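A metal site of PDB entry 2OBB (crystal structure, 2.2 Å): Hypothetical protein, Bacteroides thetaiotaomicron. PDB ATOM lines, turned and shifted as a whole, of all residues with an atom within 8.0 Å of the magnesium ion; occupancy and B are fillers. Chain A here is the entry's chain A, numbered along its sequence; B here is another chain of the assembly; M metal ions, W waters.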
ATOM      1  N   VAL A   8       2.887 -17.058 -36.347  1.00  0.00           N
ATOM      2  CA  VAL A   8       2.663 -18.425 -35.879  1.00  0.00           C
ATOM      3  C   VAL A   8       3.440 -18.710 -34.609  1.00  0.00           C
ATOM      4  O   VAL A   8       4.676 -18.570 -34.551  1.00  0.00           O
ATOM      5  CB  VAL A   8       2.994 -19.505 -36.970  1.00  0.00           C
ATOM      6  CG1 VAL A   8       2.409 -20.917 -36.547  1.00  0.00           C
ATOM      7  CG2 VAL A   8       2.455 -19.081 -38.325  1.00  0.00           C
ATOM      8  N   ASP A   9       2.715 -19.152 -33.592  1.00  0.00           N
ATOM      9  CA  ASP A   9       3.348 -19.538 -32.343  1.00  0.00           C
ATOM     10  C   ASP A   9       4.134 -20.826 -32.553  1.00  0.00           C
ATOM     11  O   ASP A   9       3.927 -21.531 -33.529  1.00  0.00           O
ATOM     12  CB  ASP A   9       2.275 -19.693 -31.280  1.00  0.00           C
ATOM     13  CG  ASP A   9       2.820 -20.194 -29.988  1.00  0.00           C
ATOM     14  OD1 ASP A   9       3.751 -19.579 -29.456  1.00  0.00           O
ATOM     15  OD2 ASP A   9       2.288 -21.198 -29.457  1.00  0.00           O
ATOM     16  N   PHE A  10       5.056 -21.126 -31.637  1.00  0.00           N
ATOM     17  CA  PHE A  10       5.789 -22.351 -31.765  1.00  0.00           C
ATOM     18  C   PHE A  10       5.263 -23.447 -30.835  1.00  0.00           C
ATOM     19  O   PHE A  10       4.620 -24.409 -31.318  1.00  0.00           O
ATOM     20  CB  PHE A  10       7.281 -22.120 -31.575  1.00  0.00           C
ATOM     21  CG  PHE A  10       8.128 -23.340 -31.837  1.00  0.00           C
ATOM     22  CD1 PHE A  10       8.191 -23.905 -33.113  1.00  0.00           C
ATOM     23  CD2 PHE A  10       8.880 -23.911 -30.818  1.00  0.00           C
ATOM     24  CE1 PHE A  10       9.000 -25.030 -33.377  1.00  0.00           C
ATOM     25  CE2 PHE A  10       9.693 -25.056 -31.073  1.00  0.00           C
ATOM     26  CZ  PHE A  10       9.745 -25.608 -32.347  1.00  0.00           C
ATOM     27  N   ASP A  11       5.512 -23.311 -29.518  1.00  0.00           N
ATOM     28  CA  ASP A  11       5.139 -24.371 -28.564  1.00  0.00           C
ATOM     29  C   ASP A  11       3.624 -24.520 -28.368  1.00  0.00           C
ATOM     30  O   ASP A  11       2.922 -23.555 -28.014  1.00  0.00           O
ATOM     31  CB  ASP A  11       5.812 -24.177 -27.211  1.00  0.00           C
ATOM     32  CG  ASP A  11       7.306 -23.986 -27.328  1.00  0.00           C
ATOM     33  OD1 ASP A  11       8.046 -24.987 -27.434  1.00  0.00           O
ATOM     34  OD2 ASP A  11       7.740 -22.811 -27.295  1.00  0.00           O
ATOM     35  N   GLY A  12       3.139 -25.737 -28.582  1.00  0.00           N
ATOM     36  CA  GLY A  12       1.717 -26.038 -28.489  1.00  0.00           C
ATOM     37  C   GLY A  12       0.981 -25.773 -29.802  1.00  0.00           C
ATOM     38  O   GLY A  12      -0.190 -26.083 -29.935  1.00  0.00           O
ATOM     39  N   THR A  13       1.694 -25.191 -30.767  1.00  0.00           N
ATOM     40  CA  THR A  13       1.119 -24.793 -32.038  1.00  0.00           C
ATOM     41  C   THR A  13       1.716 -25.572 -33.209  1.00  0.00           C
ATOM     42  O   THR A  13       0.978 -26.155 -33.996  1.00  0.00           O
ATOM     43  CB  THR A  13       1.295 -23.275 -32.291  1.00  0.00           C
ATOM     44  OG1 THR A  13       0.730 -22.553 -31.202  1.00  0.00           O
ATOM     45  CG2 THR A  13       0.600 -22.830 -33.599  1.00  0.00           C
ATOM     46  N   ILE A  14       3.042 -25.520 -33.358  1.00  0.00           N
ATOM     47  CA  ILE A  14       3.765 -26.253 -34.383  1.00  0.00           C
ATOM     48  C   ILE A  14       4.260 -27.599 -33.801  1.00  0.00           C
ATOM     49  O   ILE A  14       4.290 -28.624 -34.509  1.00  0.00           O
ATOM     50  CB  ILE A  14       4.981 -25.412 -34.929  1.00  0.00           C
ATOM     51  CG1 ILE A  14       4.489 -24.181 -35.712  1.00  0.00           C
ATOM     52  CG2 ILE A  14       5.883 -26.249 -35.851  1.00  0.00           C
ATOM     53  CD1 ILE A  14       5.605 -23.279 -36.197  1.00  0.00           C
ATOM     54  N   VAL A  15       4.657 -27.582 -32.505  1.00  0.00           N
ATOM     55  CA  VAL A  15       5.052 -28.800 -31.793  1.00  0.00           C
ATOM     56  C   VAL A  15       4.243 -28.944 -30.510  1.00  0.00           C
ATOM     57  O   VAL A  15       3.742 -27.953 -30.005  1.00  0.00           O
ATOM     58  CB  VAL A  15       6.556 -28.816 -31.448  1.00  0.00           C
ATOM     59  CG1 VAL A  15       7.373 -28.923 -32.703  1.00  0.00           C
ATOM     60  CG2 VAL A  15       6.964 -27.564 -30.627  1.00  0.00           C
ATOM     61  N   GLU A  16       4.127 -30.171 -29.981  1.00  0.00           N
ATOM     62  CA  GLU A  16       3.615 -30.363 -28.628  1.00  0.00           C
ATOM     63  C   GLU A  16       4.434 -29.496 -27.678  1.00  0.00           C
ATOM     64  O   GLU A  16       5.639 -29.296 -27.895  1.00  0.00           O
ATOM     65  CB  GLU A  16       3.761 -31.801 -28.152  1.00  0.00           C
ATOM     66  CG  GLU A  16       3.442 -32.811 -29.171  1.00  0.00           C
ATOM     67  CD  GLU A  16       2.094 -33.407 -28.971  1.00  0.00           C
ATOM     68  OE1 GLU A  16       1.092 -32.641 -29.033  1.00  0.00           O
ATOM     69  OE2 GLU A  16       2.067 -34.642 -28.731  1.00  0.00           O
ATOM     70  N   HIS A  17       3.783 -29.020 -26.617  1.00  0.00           N
ATOM     71  CA  HIS A  17       4.408 -28.082 -25.687  1.00  0.00           C
ATOM     72  C   HIS A  17       5.344 -28.811 -24.728  1.00  0.00           C
ATOM     73  O   HIS A  17       4.884 -29.403 -23.771  1.00  0.00           O
ATOM     74  CB  HIS A  17       3.317 -27.362 -24.881  1.00  0.00           C
ATOM     75  CG  HIS A  17       3.760 -26.077 -24.273  1.00  0.00           C
ATOM     76  ND1 HIS A  17       2.877 -25.081 -23.909  1.00  0.00           N
ATOM     77  CD2 HIS A  17       5.004 -25.601 -24.001  1.00  0.00           C
ATOM     78  CE1 HIS A  17       3.552 -24.053 -23.421  1.00  0.00           C
ATOM     79  NE2 HIS A  17       4.835 -24.347 -23.454  1.00  0.00           N
ATOM     80  N   TRP A  46       6.407 -16.296 -33.954  1.00  0.00           N
ATOM     81  CA  TRP A  46       5.970 -15.400 -32.875  1.00  0.00           C
ATOM     82  C   TRP A  46       5.934 -16.206 -31.599  1.00  0.00           C
ATOM     83  O   TRP A  46       4.946 -16.891 -31.332  1.00  0.00           O
ATOM     84  CB  TRP A  46       4.573 -14.865 -33.224  1.00  0.00           C
ATOM     85  CG  TRP A  46       4.004 -13.704 -32.439  1.00  0.00           C
ATOM     86  CD1 TRP A  46       2.699 -13.557 -32.106  1.00  0.00           C
ATOM     87  CD2 TRP A  46       4.692 -12.528 -31.925  1.00  0.00           C
ATOM     88  NE1 TRP A  46       2.515 -12.388 -31.424  1.00  0.00           N
ATOM     89  CE2 TRP A  46       3.709 -11.727 -31.303  1.00  0.00           C
ATOM     90  CE3 TRP A  46       6.013 -12.085 -31.927  1.00  0.00           C
ATOM     91  CZ2 TRP A  46       4.001 -10.485 -30.703  1.00  0.00           C
ATOM     92  CZ3 TRP A  46       6.321 -10.868 -31.323  1.00  0.00           C
ATOM     93  CH2 TRP A  46       5.301 -10.071 -30.717  1.00  0.00           C
ATOM     94  N   SER A  47       7.027 -16.131 -30.841  1.00  0.00           N
ATOM     95  CA  SER A  47       7.260 -16.973 -29.683  1.00  0.00           C
ATOM     96  C   SER A  47       7.856 -16.182 -28.524  1.00  0.00           C
ATOM     97  O   SER A  47       8.606 -15.231 -28.744  1.00  0.00           O
ATOM     98  CB  SER A  47       8.240 -18.075 -30.071  1.00  0.00           C
ATOM     99  OG  SER A  47       8.434 -18.979 -29.014  1.00  0.00           O
ATOM    100  N   VAL A  48       7.524 -16.567 -27.301  1.00  0.00           N
ATOM    101  CA  VAL A  48       8.184 -15.996 -26.145  1.00  0.00           C
ATOM    102  C   VAL A  48       9.656 -16.427 -26.127  1.00  0.00           C
ATOM    103  O   VAL A  48      10.460 -15.826 -25.419  1.00  0.00           O
ATOM    104  CB  VAL A  48       7.458 -16.308 -24.793  1.00  0.00           C
ATOM    105  CG1 VAL A  48       6.087 -15.627 -24.743  1.00  0.00           C
ATOM    106  CG2 VAL A  48       7.357 -17.824 -24.530  1.00  0.00           C
ATOM    107  N   ILE A  95      -1.860 -17.353 -35.336  1.00  0.00           N
ATOM    108  CA  ILE A  95      -2.145 -18.748 -35.093  1.00  0.00           C
ATOM    109  C   ILE A  95      -1.399 -19.065 -33.816  1.00  0.00           C
ATOM    110  O   ILE A  95      -0.165 -19.049 -33.799  1.00  0.00           O
ATOM    111  CB  ILE A  95      -1.666 -19.651 -36.255  1.00  0.00           C
ATOM    112  CG1 ILE A  95      -2.295 -19.184 -37.573  1.00  0.00           C
ATOM    113  CG2 ILE A  95      -1.973 -21.156 -35.962  1.00  0.00           C
ATOM    114  CD1 ILE A  95      -1.810 -19.933 -38.805  1.00  0.00           C
ATOM    115  N   ASP A  96      -2.151 -19.366 -32.765  1.00  0.00           N
ATOM    116  CA  ASP A  96      -1.593 -19.534 -31.427  1.00  0.00           C
ATOM    117  C   ASP A  96      -2.463 -20.489 -30.596  1.00  0.00           C
ATOM    118  O   ASP A  96      -3.700 -20.340 -30.529  1.00  0.00           O
ATOM    119  CB  ASP A  96      -1.564 -18.167 -30.781  1.00  0.00           C
ATOM    120  CG  ASP A  96      -0.564 -18.078 -29.657  1.00  0.00           C
ATOM    121  OD1 ASP A  96      -0.603 -19.013 -28.822  1.00  0.00           O
ATOM    122  OD2 ASP A  96       0.186 -17.030 -29.599  1.00  0.00           O
ATOM    123  N   ASP A  97      -1.851 -21.461 -29.933  1.00  0.00           N
ATOM    124  CA  ASP A  97      -2.689 -22.434 -29.196  1.00  0.00           C
ATOM    125  C   ASP A  97      -3.315 -21.776 -27.987  1.00  0.00           C
ATOM    126  O   ASP A  97      -4.225 -22.336 -27.406  1.00  0.00           O
ATOM    127  CB  ASP A  97      -1.899 -23.665 -28.793  1.00  0.00           C
ATOM    128  CG  ASP A  97      -0.775 -23.336 -27.828  1.00  0.00           C
ATOM    129  OD1 ASP A  97       0.061 -22.466 -28.178  1.00  0.00           O
ATOM    130  OD2 ASP A  97      -0.739 -23.922 -26.728  1.00  0.00           O
ATOM    131  N   ARG A  98      -2.859 -20.576 -27.632  1.00  0.00           N
ATOM    132  CA  ARG A  98      -3.444 -19.840 -26.499  1.00  0.00           C
ATOM    133  C   ARG A  98      -4.475 -18.809 -26.924  1.00  0.00           C
ATOM    134  O   ARG A  98      -4.975 -18.052 -26.102  1.00  0.00           O
ATOM    135  CB  ARG A  98      -2.388 -19.192 -25.623  1.00  0.00           C
ATOM    136  CG  ARG A  98      -1.455 -20.232 -25.011  1.00  0.00           C
ATOM    137  CD  ARG A  98      -0.453 -19.542 -24.104  1.00  0.00           C
ATOM    138  NE  ARG A  98       0.610 -20.443 -23.673  1.00  0.00           N
ATOM    139  CZ  ARG A  98       1.374 -20.235 -22.604  1.00  0.00           C
ATOM    140  NH1 ARG A  98       1.213 -19.159 -21.823  1.00  0.00           N
ATOM    141  NH2 ARG A  98       2.308 -21.118 -22.317  1.00  0.00           N
ATOM    142  N   ASN A  99      -4.803 -18.779 -28.205  1.00  0.00           N
ATOM    143  CA  ASN A  99      -5.970 -18.022 -28.659  1.00  0.00           C
ATOM    144  C   ASN A  99      -7.222 -18.518 -27.967  1.00  0.00           C
ATOM    145  O   ASN A  99      -7.435 -19.725 -27.798  1.00  0.00           O
ATOM    146  CB  ASN A  99      -6.109 -18.124 -30.178  1.00  0.00           C
ATOM    147  CG  ASN A  99      -5.038 -17.313 -30.917  1.00  0.00           C
ATOM    148  OD1 ASN A  99      -4.299 -16.563 -30.298  1.00  0.00           O
ATOM    149  ND2 ASN A  99      -4.949 -17.484 -32.195  1.00  0.00           N
ATOM    150  N   ILE A 103      -6.886 -23.557 -30.794  1.00  0.00           N
ATOM    151  CA  ILE A 103      -6.713 -23.754 -32.243  1.00  0.00           C
ATOM    152  C   ILE A 103      -7.114 -25.149 -32.705  1.00  0.00           C
ATOM    153  O   ILE A 103      -6.892 -26.135 -31.975  1.00  0.00           O
ATOM    154  CB  ILE A 103      -5.358 -23.300 -32.840  1.00  0.00           C
ATOM    155  CG1 ILE A 103      -4.177 -24.098 -32.251  1.00  0.00           C
ATOM    156  CG2 ILE A 103      -5.199 -21.626 -32.808  1.00  0.00           C
ATOM    157  CD1 ILE A 103      -2.953 -24.000 -33.228  1.00  0.00           C
ATOM    158  N   LYS B  88       7.071 -10.961 -27.289  1.00  0.00           N
ATOM    159  CA  LYS B  88       5.708 -11.448 -27.199  1.00  0.00           C
ATOM    160  C   LYS B  88       5.324 -11.577 -25.717  1.00  0.00           C
ATOM    161  O   LYS B  88       6.110 -12.085 -24.921  1.00  0.00           O
ATOM    162  CB  LYS B  88       5.609 -12.819 -27.910  1.00  0.00           C
ATOM    163  CG  LYS B  88       4.214 -13.398 -28.011  1.00  0.00           C
ATOM    164  CD  LYS B  88       4.233 -14.748 -28.721  1.00  0.00           C
ATOM    165  CE  LYS B  88       2.868 -15.428 -28.696  1.00  0.00           C
ATOM    166  NZ  LYS B  88       2.947 -16.909 -29.016  1.00  0.00           N
ATOM    167  N   ALA B  91       1.276 -13.874 -21.689  1.00  0.00           N
ATOM    168  CA  ALA B  91      -0.122 -14.147 -21.365  1.00  0.00           C
ATOM    169  C   ALA B  91      -0.553 -15.632 -21.468  1.00  0.00           C
ATOM    170  O   ALA B  91       0.010 -16.379 -22.253  1.00  0.00           O
ATOM    171  CB  ALA B  91      -1.009 -13.322 -22.253  1.00  0.00           C
ATOM    172  N   PHE B  94      -5.066 -15.198 -25.433  1.00  0.00           N
ATOM    173  CA  PHE B  94      -5.099 -14.054 -26.323  1.00  0.00           C
ATOM    174  C   PHE B  94      -6.505 -13.881 -26.914  1.00  0.00           C
ATOM    175  O   PHE B  94      -7.086 -14.791 -27.478  1.00  0.00           O
ATOM    176  CB  PHE B  94      -4.065 -14.227 -27.446  1.00  0.00           C
ATOM    177  CG  PHE B  94      -2.639 -14.237 -26.968  1.00  0.00           C
ATOM    178  CD1 PHE B  94      -2.045 -15.416 -26.521  1.00  0.00           C
ATOM    179  CD2 PHE B  94      -1.898 -13.076 -26.940  1.00  0.00           C
ATOM    180  CE1 PHE B  94      -0.715 -15.439 -26.082  1.00  0.00           C
ATOM    181  CE2 PHE B  94      -0.536 -13.067 -26.508  1.00  0.00           C
ATOM    182  CZ  PHE B  94       0.053 -14.251 -26.096  1.00  0.00           C
HETATM  183 MG    MG M   1       1.981 -21.980 -27.533  1.00  0.00          MG
HETATM  184  O   HOH W   1       1.381 -22.764 -25.661  1.00  0.00           O
HETATM  185  O   HOH W   2       1.154 -20.036 -27.325  1.00  0.00           O
HETATM  186  O   HOH W   3       3.570 -21.006 -26.762  1.00  0.00           O
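O of Asp 11 binds the magnesium ion. The magnesium ion is bound by water W3 (2.0 Å). The side-chain carboxylate (OD1) of Asp 97 is bound to the magnesium ion, 2.1 Å away. The magnesium ion is bound by the side-chain carboxylate (OD2) of Asp 9 (2.1 Å). The magnesium ion is bound by water W1 (2.1 Å). The magnesium ion is bound by water W2, at 2.1 Å.
Water W2 bridges the side-chain carboxylate (OD1) of Asp 96 and the side-chain carboxylate (OD1) of Asp 9. Water W1 lies within hydrogen-bond range of OD2 of Asp 97 (2.6 Å), NE of Arg 98 (3.2 Å) and ND1 of His 17 (3.3 Å).
Thr 13 touches the magnesium ion (OG1 to MG, 3.9 Å).
N of Asp 9 sits at hydrogen-bond distance from O of Ile 95 (2.9 Å). The side-chain carboxylate of Asp 9 lies close to the side-chain hydroxyl of Thr 13, 2.7 Å away. The side-chain carboxylate of Asp 9 lies within salt-bridge range of the side-chain amino group of Lys 88 of chain B (2.8 Å). The side-chain hydroxyl (OG1) of Thr 13 lies within hydrogen-bond range of the backbone NH (N) of Asp 97 (3.1 Å).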
